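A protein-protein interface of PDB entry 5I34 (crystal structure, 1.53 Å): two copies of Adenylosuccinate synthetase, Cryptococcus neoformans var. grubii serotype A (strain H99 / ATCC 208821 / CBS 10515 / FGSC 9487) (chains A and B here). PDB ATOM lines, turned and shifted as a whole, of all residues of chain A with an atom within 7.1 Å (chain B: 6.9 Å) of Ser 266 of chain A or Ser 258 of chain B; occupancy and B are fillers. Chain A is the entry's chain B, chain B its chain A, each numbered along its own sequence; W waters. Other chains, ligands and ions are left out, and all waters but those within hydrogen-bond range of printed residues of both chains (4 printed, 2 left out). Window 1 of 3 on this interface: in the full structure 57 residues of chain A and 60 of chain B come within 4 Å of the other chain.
The side-chain hydroxyl of Ser 258 of chain B is in hydrogen-bond range of the side-chain hydroxyl of Ser 260 of chain B.
OG of Ser 258 of chain B sits close to OD1 of Asp 245 of chain B.
The backbone NH of Gly 263 of chain B lies within hydrogen-bond range of the side-chain hydroxyl of Ser 258 of chain B (3.1 Å).
The backbone carbonyl oxygen (O) of Gly 262 of chain B sits at hydrogen-bond distance from the side-chain hydroxyl (OG) of Ser 266 of chain B, at 3.4 Å.
OG of Ser 266 of chain A is in hydrogen-bond range of O of Gly 262 of chain A (3.4 Å).
OD2 of Asp 245 of chain B lies within hydrogen-bond range of N of Asp 247 of chain B, at 2.9 Å.
Hydrophobic or aromatic side chains of chain A within 4 Å of the printed part of chain B: Ile 261 and Val 265.
Along chain A the printed residues that touch a printed residue of chain B span positions 91 to 270.
Of the 25 printed residues of chain B, 9 touch a printed residue of chain A.
Printed residues of chain B that touch a printed residue of chain A: Asp 247, Tyr 248, Ser 258, Ile 261, Gly 262, Gly 263, Val 265, Ser 266 and Ile 337.
Hydrophobic or aromatic side chains of chain B that line the printed part of chain A: Tyr 248, Ile 261, Val 265 and Ile 337.
Among the printed residues, no Asp or Glu carboxylate lies within 4 Å of a Lys or Arg side-chain nitrogen of the other chain.
O of Ser 266 of chain A sits at hydrogen-bond distance from OH of Tyr 248 of chain B (2.7 Å).
OH of Tyr 248 of chain B sits at hydrogen-bond distance from N of Gly 269 of chain A.
OH of Tyr 248 of chain B lies within hydrogen-bond range of O of Gly 267 of chain A (3.3 Å).
Printed residues of chain B within 4 Å of Ile 261 of chain A: Val 265.
Of chain B, only Tyr 248, Ser 258, Gly 262 and Gly 263 come within 4 Å of Ser 266 of chain A.
Printed residues of chain B within 4 Å of Gly 269 of chain A: Tyr 248 and Ile 337.
Ala 241 of chain B touches none of the printed residues of chain A.
Ser 258 of chain B touches one residue of chain A.
Of the printed residues of chain A, Ile 261 of chain B touches Val 265.
The nearest residue of chain A that does not touch Ser 258 of chain B is Gly 262 of chain A (6.7 Å).
Among the printed residues, pairs that only touch across the chains: Gly 262 of chain A with Ser 266 of chain B (3.2 Å), Ser 266 of chain A with Gly 262 of chain B (3.3 Å), Val 265 of chain A with Gly 262 of chain B (3.3 Å), Gly 269 of chain A with Ile 337 of chain B (3.3 Å), Leu 268 of chain A with Tyr 248 of chain B (3.4 Å), Gly 262 of chain A with Val 265 of chain B (3.5 Å), Ser 266 of chain A with Ser 258 of chain B (3.5 Å), Ser 91 of chain A with Tyr 248 of chain B (3.6 Å), Ser 91 of chain A with Asp 247 of chain B (3.6 Å), Ile 270 of chain A with Ile 337 of chain B (3.7 Å), Gly 263 of chain A with Ser 266 of chain B (3.7 Å), Ser 266 of chain A with Gly 263 of chain B (3.7 Å), Ser 258 of chain A with Ser 266 of chain B (3.9 Å), Val 265 of chain A with Ile 261 of chain B (3.9 Å), Ile 261 of chain A with Val 265 of chain B (3.98 Å) and Gly 262 of chain A with Gly 262 of chain B (3.996 Å).
Water W2 lies within hydrogen-bond range of the side-chain hydroxyl (OG) of Ser 91 of chain A, the side-chain hydroxyl (OH) of Tyr 248 of chain B and the backbone carbonyl oxygen (O) of Gly 267 of chain A.
Water W3 bridges OD1 of Asp 247 of chain B and O of Ser 91 of chain A.
Water W1 lies within hydrogen-bond range of OG of Ser 266 of chain B (2.7 Å) and OG of Ser 266 of chain A (2.8 Å).
Water W4 lies within hydrogen-bond range of the side-chain carboxylate (OD2) of Asp 247 of chain B (2.8 Å) and the backbone NH (N) of Gly 267 of chain A (3.5 Å).
Ser 258 of chain A touches Ser 266 of chain B, and with the chains exchanged Ser 266 of chain A touches Ser 258 of chain B.
Ile 261 of chain A touches Val 265 of chain B, and with the chains exchanged Val 265 of chain A touches Ile 261 of chain B.
Gly 262 of chain B touches its own counterpart, Gly 262 of chain A.
Gly 262 of chain A touches Val 265 of chain B, and with the chains exchanged Val 265 of chain A touches Gly 262 of chain B.
8 positions are printed for both chains.
Of the 19 pairs that touch across the chains among the printed residues, 11 have their exchanged pair printed and touching as well.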
ATOM      1  N   CYS A  49     -22.728  12.817 -19.543  1.00  0.00           N
ATOM      2  CA  CYS A  49     -23.565  13.360 -20.621  1.00  0.00           C
ATOM      3  C   CYS A  49     -23.657  12.441 -21.826  1.00  0.00           C
ATOM      4  O   CYS A  49     -24.614  12.527 -22.580  1.00  0.00           O
ATOM      5  CB  CYS A  49     -23.043  14.743 -21.046  1.00  0.00           C
ATOM      6  SG  CYS A  49     -21.311  14.793 -21.537  1.00  0.00           S
ATOM      7  N   GLY A  90     -27.165  11.725 -17.806  1.00  0.00           N
ATOM      8  CA  GLY A  90     -27.906  12.481 -18.802  1.00  0.00           C
ATOM      9  C   GLY A  90     -28.542  11.657 -19.909  1.00  0.00           C
ATOM     10  O   GLY A  90     -28.308  10.443 -20.033  1.00  0.00           O
ATOM     11  N   SER A  91     -29.349  12.320 -20.733  1.00  0.00           N
ATOM     12  CA  SER A  91     -30.099  11.652 -21.788  1.00  0.00           C
ATOM     13  C   SER A  91     -29.213  11.098 -22.891  1.00  0.00           C
ATOM     14  O   SER A  91     -29.624  10.199 -23.624  1.00  0.00           O
ATOM     15  CB  SER A  91     -31.114  12.631 -22.391  1.00  0.00           C
ATOM     16  OG  SER A  91     -32.017  13.080 -21.405  1.00  0.00           O
ATOM     17  N   GLY A  92     -28.014  11.653 -23.026  1.00  0.00           N
ATOM     18  CA  GLY A  92     -27.091  11.255 -24.082  1.00  0.00           C
ATOM     19  C   GLY A  92     -26.314   9.967 -23.854  1.00  0.00           C
ATOM     20  O   GLY A  92     -25.603   9.505 -24.745  1.00  0.00           O
ATOM     21  N   SER A 258     -20.609  11.694 -29.305  1.00  0.00           N
ATOM     22  CA  SER A 258     -19.846  12.885 -29.179  1.00  0.00           C
ATOM     23  C   SER A 258     -19.128  12.927 -27.841  1.00  0.00           C
ATOM     24  O   SER A 258     -19.741  13.072 -26.790  1.00  0.00           O
ATOM     25  CB  SER A 258     -20.741  14.095 -29.301  1.00  0.00           C
ATOM     26  OG  SER A 258     -19.998  15.196 -28.827  1.00  0.00           O
ATOM     27  N   ILE A 261     -17.209  18.794 -26.682  1.00  0.00           N
ATOM     28  CA  ILE A 261     -18.011  19.749 -25.910  1.00  0.00           C
ATOM     29  C   ILE A 261     -19.480  19.802 -26.364  1.00  0.00           C
ATOM     30  O   ILE A 261     -20.382  19.957 -25.524  1.00  0.00           O
ATOM     31  CB  ILE A 261     -17.348  21.153 -25.925  1.00  0.00           C
ATOM     32  CG1 ILE A 261     -18.055  22.116 -24.970  1.00  0.00           C
ATOM     33  CG2 ILE A 261     -17.251  21.736 -27.328  1.00  0.00           C
ATOM     34  CD1 ILE A 261     -18.083  21.684 -23.492  1.00  0.00           C
ATOM     35  N   GLY A 262     -19.756  19.612 -27.655  1.00  0.00           N
ATOM     36  CA  GLY A 262     -21.133  19.596 -28.112  1.00  0.00           C
ATOM     37  C   GLY A 262     -21.958  18.479 -27.494  1.00  0.00           C
ATOM     38  O   GLY A 262     -23.176  18.578 -27.364  1.00  0.00           O
ATOM     39  N   GLY A 263     -21.286  17.394 -27.129  1.00  0.00           N
ATOM     40  CA  GLY A 263     -21.925  16.254 -26.497  1.00  0.00           C
ATOM     41  C   GLY A 263     -22.392  16.564 -25.092  1.00  0.00           C
ATOM     42  O   GLY A 263     -23.280  15.910 -24.558  1.00  0.00           O
ATOM     43  N   VAL A 264     -21.793  17.584 -24.483  1.00  0.00           N
ATOM     44  CA  VAL A 264     -22.225  18.051 -23.172  1.00  0.00           C
ATOM     45  C   VAL A 264     -23.530  18.806 -23.339  1.00  0.00           C
ATOM     46  O   VAL A 264     -24.510  18.594 -22.612  1.00  0.00           O
ATOM     47  CB  VAL A 264     -21.170  18.968 -22.531  1.00  0.00           C
ATOM     48  CG1 VAL A 264     -21.680  19.527 -21.198  1.00  0.00           C
ATOM     49  CG2 VAL A 264     -19.844  18.221 -22.374  1.00  0.00           C
ATOM     50  N   VAL A 265     -23.546  19.692 -24.314  1.00  0.00           N
ATOM     51  CA  VAL A 265     -24.745  20.494 -24.602  1.00  0.00           C
ATOM     52  C   VAL A 265     -25.919  19.583 -24.976  1.00  0.00           C
ATOM     53  O   VAL A 265     -27.018  19.690 -24.401  1.00  0.00           O
ATOM     54  CB  VAL A 265     -24.466  21.510 -25.722  1.00  0.00           C
ATOM     55  CG1 VAL A 265     -25.716  22.300 -26.095  1.00  0.00           C
ATOM     56  CG2 VAL A 265     -23.338  22.462 -25.278  1.00  0.00           C
ATOM     57  N   SER A 266     -25.702  18.682 -25.926  1.00  0.00           N
ATOM     58  CA  SER A 266     -26.747  17.741 -26.326  1.00  0.00           C
ATOM     59  C   SER A 266     -27.097  16.733 -25.241  1.00  0.00           C
ATOM     60  O   SER A 266     -28.261  16.443 -24.996  1.00  0.00           O
ATOM     61  CB  SER A 266     -26.319  16.978 -27.576  1.00  0.00           C
ATOM     62  OG  SER A 266     -26.255  17.863 -28.668  1.00  0.00           O
ATOM     63  N   GLY A 267     -26.080  16.174 -24.597  1.00  0.00           N
ATOM     64  CA  GLY A 267     -26.287  15.074 -23.669  1.00  0.00           C
ATOM     65  C   GLY A 267     -27.006  15.480 -22.406  1.00  0.00           C
ATOM     66  O   GLY A 267     -27.679  14.651 -21.779  1.00  0.00           O
ATOM     67  N   LEU A 268     -26.880  16.757 -22.033  1.00  0.00           N
ATOM     68  CA  LEU A 268     -27.596  17.297 -20.870  1.00  0.00           C
ATOM     69  C   LEU A 268     -28.773  18.199 -21.211  1.00  0.00           C
ATOM     70  O   LEU A 268     -29.563  18.558 -20.315  1.00  0.00           O
ATOM     71  CB  LEU A 268     -26.635  18.089 -19.984  1.00  0.00           C
ATOM     72  CG  LEU A 268     -25.407  17.327 -19.489  1.00  0.00           C
ATOM     73  CD1 LEU A 268     -24.538  18.226 -18.568  1.00  0.00           C
ATOM     74  CD2 LEU A 268     -25.821  16.069 -18.742  1.00  0.00           C
ATOM     75  N   GLY A 269     -28.882  18.582 -22.478  1.00  0.00           N
ATOM     76  CA  GLY A 269     -30.012  19.373 -22.923  1.00  0.00           C
ATOM     77  C   GLY A 269     -30.007  20.747 -22.286  1.00  0.00           C
ATOM     78  O   GLY A 269     -31.040  21.243 -21.814  1.00  0.00           O
ATOM     79  N   ILE A 270     -28.829  21.358 -22.254  1.00  0.00           N
ATOM     80  CA  ILE A 270     -28.645  22.683 -21.682  1.00  0.00           C
ATOM     81  C   ILE A 270     -28.235  23.693 -22.748  1.00  0.00           C
ATOM     82  O   ILE A 270     -27.793  23.328 -23.831  1.00  0.00           O
ATOM     83  CB  ILE A 270     -27.561  22.685 -20.567  1.00  0.00           C
ATOM     84  CG1 ILE A 270     -26.198  22.214 -21.123  1.00  0.00           C
ATOM     85  CG2 ILE A 270     -28.023  21.855 -19.361  1.00  0.00           C
ATOM     86  CD1 ILE A 270     -25.064  22.243 -20.117  1.00  0.00           C
ATOM     87  N   CYS B  49     -25.583  22.602 -40.095  1.00  0.00           N
ATOM     88  CA  CYS B  49     -24.799  21.874 -39.090  1.00  0.00           C
ATOM     89  C   CYS B  49     -25.200  20.411 -38.917  1.00  0.00           C
ATOM     90  O   CYS B  49     -24.399  19.602 -38.473  1.00  0.00           O
ATOM     91  CB  CYS B  49     -24.894  22.575 -37.742  1.00  0.00           C
ATOM     92  SG  CYS B  49     -26.568  22.788 -37.119  1.00  0.00           S
ATOM     93  N   ALA B  50     -26.451  20.079 -39.214  1.00  0.00           N
ATOM     94  CA  ALA B  50     -26.925  18.716 -39.039  1.00  0.00           C
ATOM     95  C   ALA B  50     -28.131  18.469 -39.922  1.00  0.00           C
ATOM     96  O   ALA B  50     -28.669  19.400 -40.536  1.00  0.00           O
ATOM     97  CB  ALA B  50     -27.266  18.460 -37.604  1.00  0.00           C
ATOM     98  N   GLY B  51     -28.578  17.214 -39.948  1.00  0.00           N
ATOM     99  CA  GLY B  51     -29.701  16.838 -40.784  1.00  0.00           C
ATOM    100  C   GLY B  51     -29.310  16.570 -42.220  1.00  0.00           C
ATOM    101  O   GLY B  51     -28.128  16.535 -42.567  1.00  0.00           O
ATOM    102  N   TYR B 158     -27.504   8.041 -40.603  1.00  0.00           N
ATOM    103  CA  TYR B 158     -27.048   8.292 -39.236  1.00  0.00           C
ATOM    104  C   TYR B 158     -26.794   6.979 -38.479  1.00  0.00           C
ATOM    105  O   TYR B 158     -25.926   6.939 -37.611  1.00  0.00           O
ATOM    106  CB  TYR B 158     -28.050   9.181 -38.477  1.00  0.00           C
ATOM    107  CG  TYR B 158     -27.839  10.667 -38.744  1.00  0.00           C
ATOM    108  CD1 TYR B 158     -26.680  11.294 -38.319  1.00  0.00           C
ATOM    109  CD2 TYR B 158     -28.779  11.426 -39.433  1.00  0.00           C
ATOM    110  CE1 TYR B 158     -26.483  12.643 -38.561  1.00  0.00           C
ATOM    111  CE2 TYR B 158     -28.580  12.766 -39.682  1.00  0.00           C
ATOM    112  CZ  TYR B 158     -27.430  13.360 -39.255  1.00  0.00           C
ATOM    113  OH  TYR B 158     -27.218  14.697 -39.508  1.00  0.00           O
ATOM    114  N   ALA B 239     -32.098  22.681 -39.153  1.00  0.00           N
ATOM    115  CA  ALA B 239     -33.061  21.890 -39.893  1.00  0.00           C
ATOM    116  C   ALA B 239     -34.032  21.246 -38.920  1.00  0.00           C
ATOM    117  O   ALA B 239     -33.720  21.045 -37.737  1.00  0.00           O
ATOM    118  CB  ALA B 239     -32.356  20.834 -40.757  1.00  0.00           C
ATOM    119  N   ASN B 240     -35.218  20.931 -39.423  1.00  0.00           N
ATOM    120  CA  ASN B 240     -36.239  20.309 -38.608  1.00  0.00           C
ATOM    121  C   ASN B 240     -36.555  21.200 -37.404  1.00  0.00           C
ATOM    122  O   ASN B 240     -36.615  22.426 -37.540  1.00  0.00           O
ATOM    123  CB  ASN B 240     -35.773  18.907 -38.202  1.00  0.00           C
ATOM    124  CG  ASN B 240     -35.059  18.169 -39.343  1.00  0.00           C
ATOM    125  OD1 ASN B 240     -33.838  17.948 -39.319  1.00  0.00           O
ATOM    126  ND2 ASN B 240     -35.812  17.813 -40.354  1.00  0.00           N
ATOM    127  N   ALA B 241     -36.731  20.614 -36.220  1.00  0.00           N
ATOM    128  CA  ALA B 241     -37.175  21.384 -35.051  1.00  0.00           C
ATOM    129  C   ALA B 241     -36.982  20.604 -33.765  1.00  0.00           C
ATOM    130  O   ALA B 241     -36.732  19.406 -33.803  1.00  0.00           O
ATOM    131  CB  ALA B 241     -38.638  21.787 -35.218  1.00  0.00           C
ATOM    132  N   LEU B 244     -38.485  17.248 -32.815  1.00  0.00           N
ATOM    133  CA  LEU B 244     -37.975  16.171 -33.662  1.00  0.00           C
ATOM    134  C   LEU B 244     -36.526  15.788 -33.304  1.00  0.00           C
ATOM    135  O   LEU B 244     -35.915  14.966 -33.984  1.00  0.00           O
ATOM    136  CB  LEU B 244     -38.042  16.575 -35.136  1.00  0.00           C
ATOM    137  CG  LEU B 244     -39.446  16.861 -35.647  1.00  0.00           C
ATOM    138  CD1 LEU B 244     -39.393  17.489 -37.031  1.00  0.00           C
ATOM    139  CD2 LEU B 244     -40.310  15.578 -35.657  1.00  0.00           C
ATOM    140  N   ASP B 245     -35.983  16.365 -32.248  1.00  0.00           N
ATOM    141  CA  ASP B 245     -34.602  16.072 -31.815  1.00  0.00           C
ATOM    142  C   ASP B 245     -34.479  14.594 -31.414  1.00  0.00           C
ATOM    143  O   ASP B 245     -35.345  14.072 -30.718  1.00  0.00           O
ATOM    144  CB  ASP B 245     -34.225  16.976 -30.642  1.00  0.00           C
ATOM    145  CG  ASP B 245     -32.805  16.826 -30.227  1.00  0.00           C
ATOM    146  OD1 ASP B 245     -31.951  17.524 -30.813  1.00  0.00           O
ATOM    147  OD2 ASP B 245     -32.533  16.021 -29.326  1.00  0.00           O
ATOM    148  N   LEU B 246     -33.390  13.939 -31.808  1.00  0.00           N
ATOM    149  CA  LEU B 246     -33.215  12.514 -31.529  1.00  0.00           C
ATOM    150  C   LEU B 246     -33.285  12.233 -30.028  1.00  0.00           C
ATOM    151  O   LEU B 246     -33.893  11.235 -29.618  1.00  0.00           O
ATOM    152  CB  LEU B 246     -31.889  12.011 -32.117  1.00  0.00           C
ATOM    153  CG  LEU B 246     -31.569  10.529 -31.900  1.00  0.00           C
ATOM    154  CD1 LEU B 246     -32.710   9.617 -32.365  1.00  0.00           C
ATOM    155  CD2 LEU B 246     -30.267  10.143 -32.541  1.00  0.00           C
ATOM    156  N   ASP B 247     -32.669  13.098 -29.209  1.00  0.00           N
ATOM    157  CA  ASP B 247     -32.722  12.943 -27.757  1.00  0.00           C
ATOM    158  C   ASP B 247     -34.008  13.491 -27.152  1.00  0.00           C
ATOM    159  O   ASP B 247     -34.640  12.814 -26.346  1.00  0.00           O
ATOM    160  CB  ASP B 247     -31.534  13.639 -27.066  1.00  0.00           C
ATOM    161  CG  ASP B 247     -30.212  12.956 -27.334  1.00  0.00           C
ATOM    162  OD1 ASP B 247     -30.034  11.810 -26.842  1.00  0.00           O
ATOM    163  OD2 ASP B 247     -29.353  13.572 -28.005  1.00  0.00           O
ATOM    164  N   TYR B 248     -34.407  14.706 -27.536  1.00  0.00           N
ATOM    165  CA  TYR B 248     -35.433  15.437 -26.763  1.00  0.00           C
ATOM    166  C   TYR B 248     -36.833  15.501 -27.381  1.00  0.00           C
ATOM    167  O   TYR B 248     -37.757  15.935 -26.720  1.00  0.00           O
ATOM    168  CB  TYR B 248     -34.910  16.865 -26.451  1.00  0.00           C
ATOM    169  CG  TYR B 248     -33.679  16.714 -25.609  1.00  0.00           C
ATOM    170  CD1 TYR B 248     -33.763  16.109 -24.365  1.00  0.00           C
ATOM    171  CD2 TYR B 248     -32.435  17.093 -26.068  1.00  0.00           C
ATOM    172  CE1 TYR B 248     -32.646  15.878 -23.603  1.00  0.00           C
ATOM    173  CE2 TYR B 248     -31.292  16.863 -25.312  1.00  0.00           C
ATOM    174  CZ  TYR B 248     -31.412  16.258 -24.067  1.00  0.00           C
ATOM    175  OH  TYR B 248     -30.307  15.985 -23.310  1.00  0.00           O
ATOM    176  N   THR B 255     -36.404  12.800 -35.844  1.00  0.00           N
ATOM    177  CA  THR B 255     -35.365  12.585 -36.828  1.00  0.00           C
ATOM    178  C   THR B 255     -34.104  12.108 -36.086  1.00  0.00           C
ATOM    179  O   THR B 255     -34.088  12.048 -34.850  1.00  0.00           O
ATOM    180  CB  THR B 255     -35.112  13.860 -37.666  1.00  0.00           C
ATOM    181  OG1 THR B 255     -34.303  13.539 -38.804  1.00  0.00           O
ATOM    182  CG2 THR B 255     -34.432  14.916 -36.861  1.00  0.00           C
ATOM    183  N   SER B 256     -33.080  11.715 -36.841  1.00  0.00           N
ATOM    184  CA  SER B 256     -31.944  10.996 -36.281  1.00  0.00           C
ATOM    185  C   SER B 256     -30.714  11.863 -36.039  1.00  0.00           C
ATOM    186  O   SER B 256     -29.618  11.338 -35.878  1.00  0.00           O
ATOM    187  CB  SER B 256     -31.584   9.846 -37.199  1.00  0.00           C
ATOM    188  OG  SER B 256     -32.697   8.979 -37.285  1.00  0.00           O
ATOM    189  N   SER B 257     -30.915  13.176 -35.996  1.00  0.00           N
ATOM    190  CA  SER B 257     -29.847  14.132 -35.708  1.00  0.00           C
ATOM    191  C   SER B 257     -30.274  14.942 -34.498  1.00  0.00           C
ATOM    192  O   SER B 257     -31.439  14.931 -34.122  1.00  0.00           O
ATOM    193  CB  SER B 257     -29.579  15.063 -36.906  1.00  0.00           C
ATOM    194  OG  SER B 257     -30.695  15.890 -37.202  1.00  0.00           O
ATOM    195  N   SER B 258     -29.313  15.636 -33.904  1.00  0.00           N
ATOM    196  CA  SER B 258     -29.603  16.650 -32.933  1.00  0.00           C
ATOM    197  C   SER B 258     -30.053  17.918 -33.647  1.00  0.00           C
ATOM    198  O   SER B 258     -29.228  18.640 -34.227  1.00  0.00           O
ATOM    199  CB  SER B 258     -28.379  16.919 -32.067  1.00  0.00           C
ATOM    200  OG  SER B 258     -28.614  18.086 -31.310  1.00  0.00           O
ATOM    201  N   THR B 259     -31.361  18.179 -33.590  1.00  0.00           N
ATOM    202  CA  THR B 259     -31.960  19.378 -34.178  1.00  0.00           C
ATOM    203  C   THR B 259     -31.866  20.574 -33.236  1.00  0.00           C
ATOM    204  O   THR B 259     -32.210  21.698 -33.591  1.00  0.00           O
ATOM    205  CB  THR B 259     -33.421  19.146 -34.461  1.00  0.00           C
ATOM    206  OG1 THR B 259     -34.066  18.898 -33.205  1.00  0.00           O
ATOM    207  CG2 THR B 259     -33.622  17.955 -35.410  1.00  0.00           C
ATOM    208  N   SER B 260     -31.426  20.307 -32.020  1.00  0.00           N
ATOM    209  CA  SER B 260     -31.336  21.297 -30.955  1.00  0.00           C
ATOM    210  C   SER B 260     -29.959  21.990 -30.987  1.00  0.00           C
ATOM    211  O   SER B 260     -29.111  21.692 -31.826  1.00  0.00           O
ATOM    212  CB  SER B 260     -31.582  20.618 -29.613  1.00  0.00           C
ATOM    213  OG  SER B 260     -30.702  19.539 -29.400  1.00  0.00           O
ATOM    214  N   ILE B 261     -29.756  22.917 -30.061  1.00  0.00           N
ATOM    215  CA  ILE B 261     -28.591  23.792 -30.096  1.00  0.00           C
ATOM    216  C   ILE B 261     -27.274  23.016 -29.977  1.00  0.00           C
ATOM    217  O   ILE B 261     -26.274  23.419 -30.571  1.00  0.00           O
ATOM    218  CB  ILE B 261     -28.714  24.862 -28.991  1.00  0.00           C
ATOM    219  CG1 ILE B 261     -27.590  25.919 -29.082  1.00  0.00           C
ATOM    220  CG2 ILE B 261     -28.798  24.211 -27.612  1.00  0.00           C
ATOM    221  CD1 ILE B 261     -27.522  26.644 -30.422  1.00  0.00           C
ATOM    222  N   GLY B 262     -27.264  21.891 -29.260  1.00  0.00           N
ATOM    223  CA  GLY B 262     -26.056  21.092 -29.175  1.00  0.00           C
ATOM    224  C   GLY B 262     -25.595  20.555 -30.527  1.00  0.00           C
ATOM    225  O   GLY B 262     -24.408  20.327 -30.739  1.00  0.00           O
ATOM    226  N   GLY B 263     -26.525  20.357 -31.449  1.00  0.00           N
ATOM    227  CA  GLY B 263     -26.183  19.917 -32.792  1.00  0.00           C
ATOM    228  C   GLY B 263     -25.449  20.957 -33.605  1.00  0.00           C
ATOM    229  O   GLY B 263     -24.769  20.632 -34.586  1.00  0.00           O
ATOM    230  N   VAL B 264     -25.590  22.212 -33.210  1.00  0.00           N
ATOM    231  CA  VAL B 264     -24.815  23.297 -33.808  1.00  0.00           C
ATOM    232  C   VAL B 264     -23.362  23.200 -33.355  1.00  0.00           C
ATOM    233  O   VAL B 264     -22.421  23.257 -34.176  1.00  0.00           O
ATOM    234  CB  VAL B 264     -25.381  24.684 -33.422  1.00  0.00           C
ATOM    235  CG1 VAL B 264     -24.528  25.788 -34.000  1.00  0.00           C
ATOM    236  CG2 VAL B 264     -26.810  24.808 -33.866  1.00  0.00           C
ATOM    237  N   VAL B 265     -23.169  23.065 -32.048  1.00  0.00           N
ATOM    238  CA  VAL B 265     -21.839  22.963 -31.476  1.00  0.00           C
ATOM    239  C   VAL B 265     -21.116  21.738 -32.040  1.00  0.00           C
ATOM    240  O   VAL B 265     -19.982  21.840 -32.515  1.00  0.00           O
ATOM    241  CB  VAL B 265     -21.913  22.899 -29.919  1.00  0.00           C
ATOM    242  CG1 VAL B 265     -20.535  22.806 -29.300  1.00  0.00           C
ATOM    243  CG2 VAL B 265     -22.654  24.119 -29.357  1.00  0.00           C
ATOM    244  N   SER B 266     -21.762  20.576 -31.994  1.00  0.00           N
ATOM    245  CA  SER B 266     -21.160  19.344 -32.517  1.00  0.00           C
ATOM    246  C   SER B 266     -21.005  19.374 -34.019  1.00  0.00           C
ATOM    247  O   SER B 266     -19.971  18.980 -34.585  1.00  0.00           O
ATOM    248  CB  SER B 266     -22.017  18.124 -32.135  1.00  0.00           C
ATOM    249  OG  SER B 266     -22.017  17.910 -30.733  1.00  0.00           O
ATOM    250  N   ILE B 337     -34.413  23.655 -23.377  1.00  0.00           N
ATOM    251  CA  ILE B 337     -33.353  22.914 -24.055  1.00  0.00           C
ATOM    252  C   ILE B 337     -32.501  23.819 -24.940  1.00  0.00           C
ATOM    253  O   ILE B 337     -31.264  23.713 -24.968  1.00  0.00           O
ATOM    254  CB  ILE B 337     -33.936  21.758 -24.935  1.00  0.00           C
ATOM    255  CG1 ILE B 337     -34.684  20.730 -24.059  1.00  0.00           C
ATOM    256  CG2 ILE B 337     -32.841  21.073 -25.745  1.00  0.00           C
ATOM    257  CD1 ILE B 337     -33.813  19.968 -23.141  1.00  0.00           C
HETATM  258  O   HOH W   1     -24.317  16.590 -30.245  1.00  0.00           O
HETATM  259  O   HOH W   2     -30.682  15.146 -20.596  1.00  0.00           O
HETATM  260  O   HOH W   3     -31.794  10.073 -25.797  1.00  0.00           O
HETATM  261  O   HOH W   4     -26.773  13.659 -26.862  1.00  0.00           O
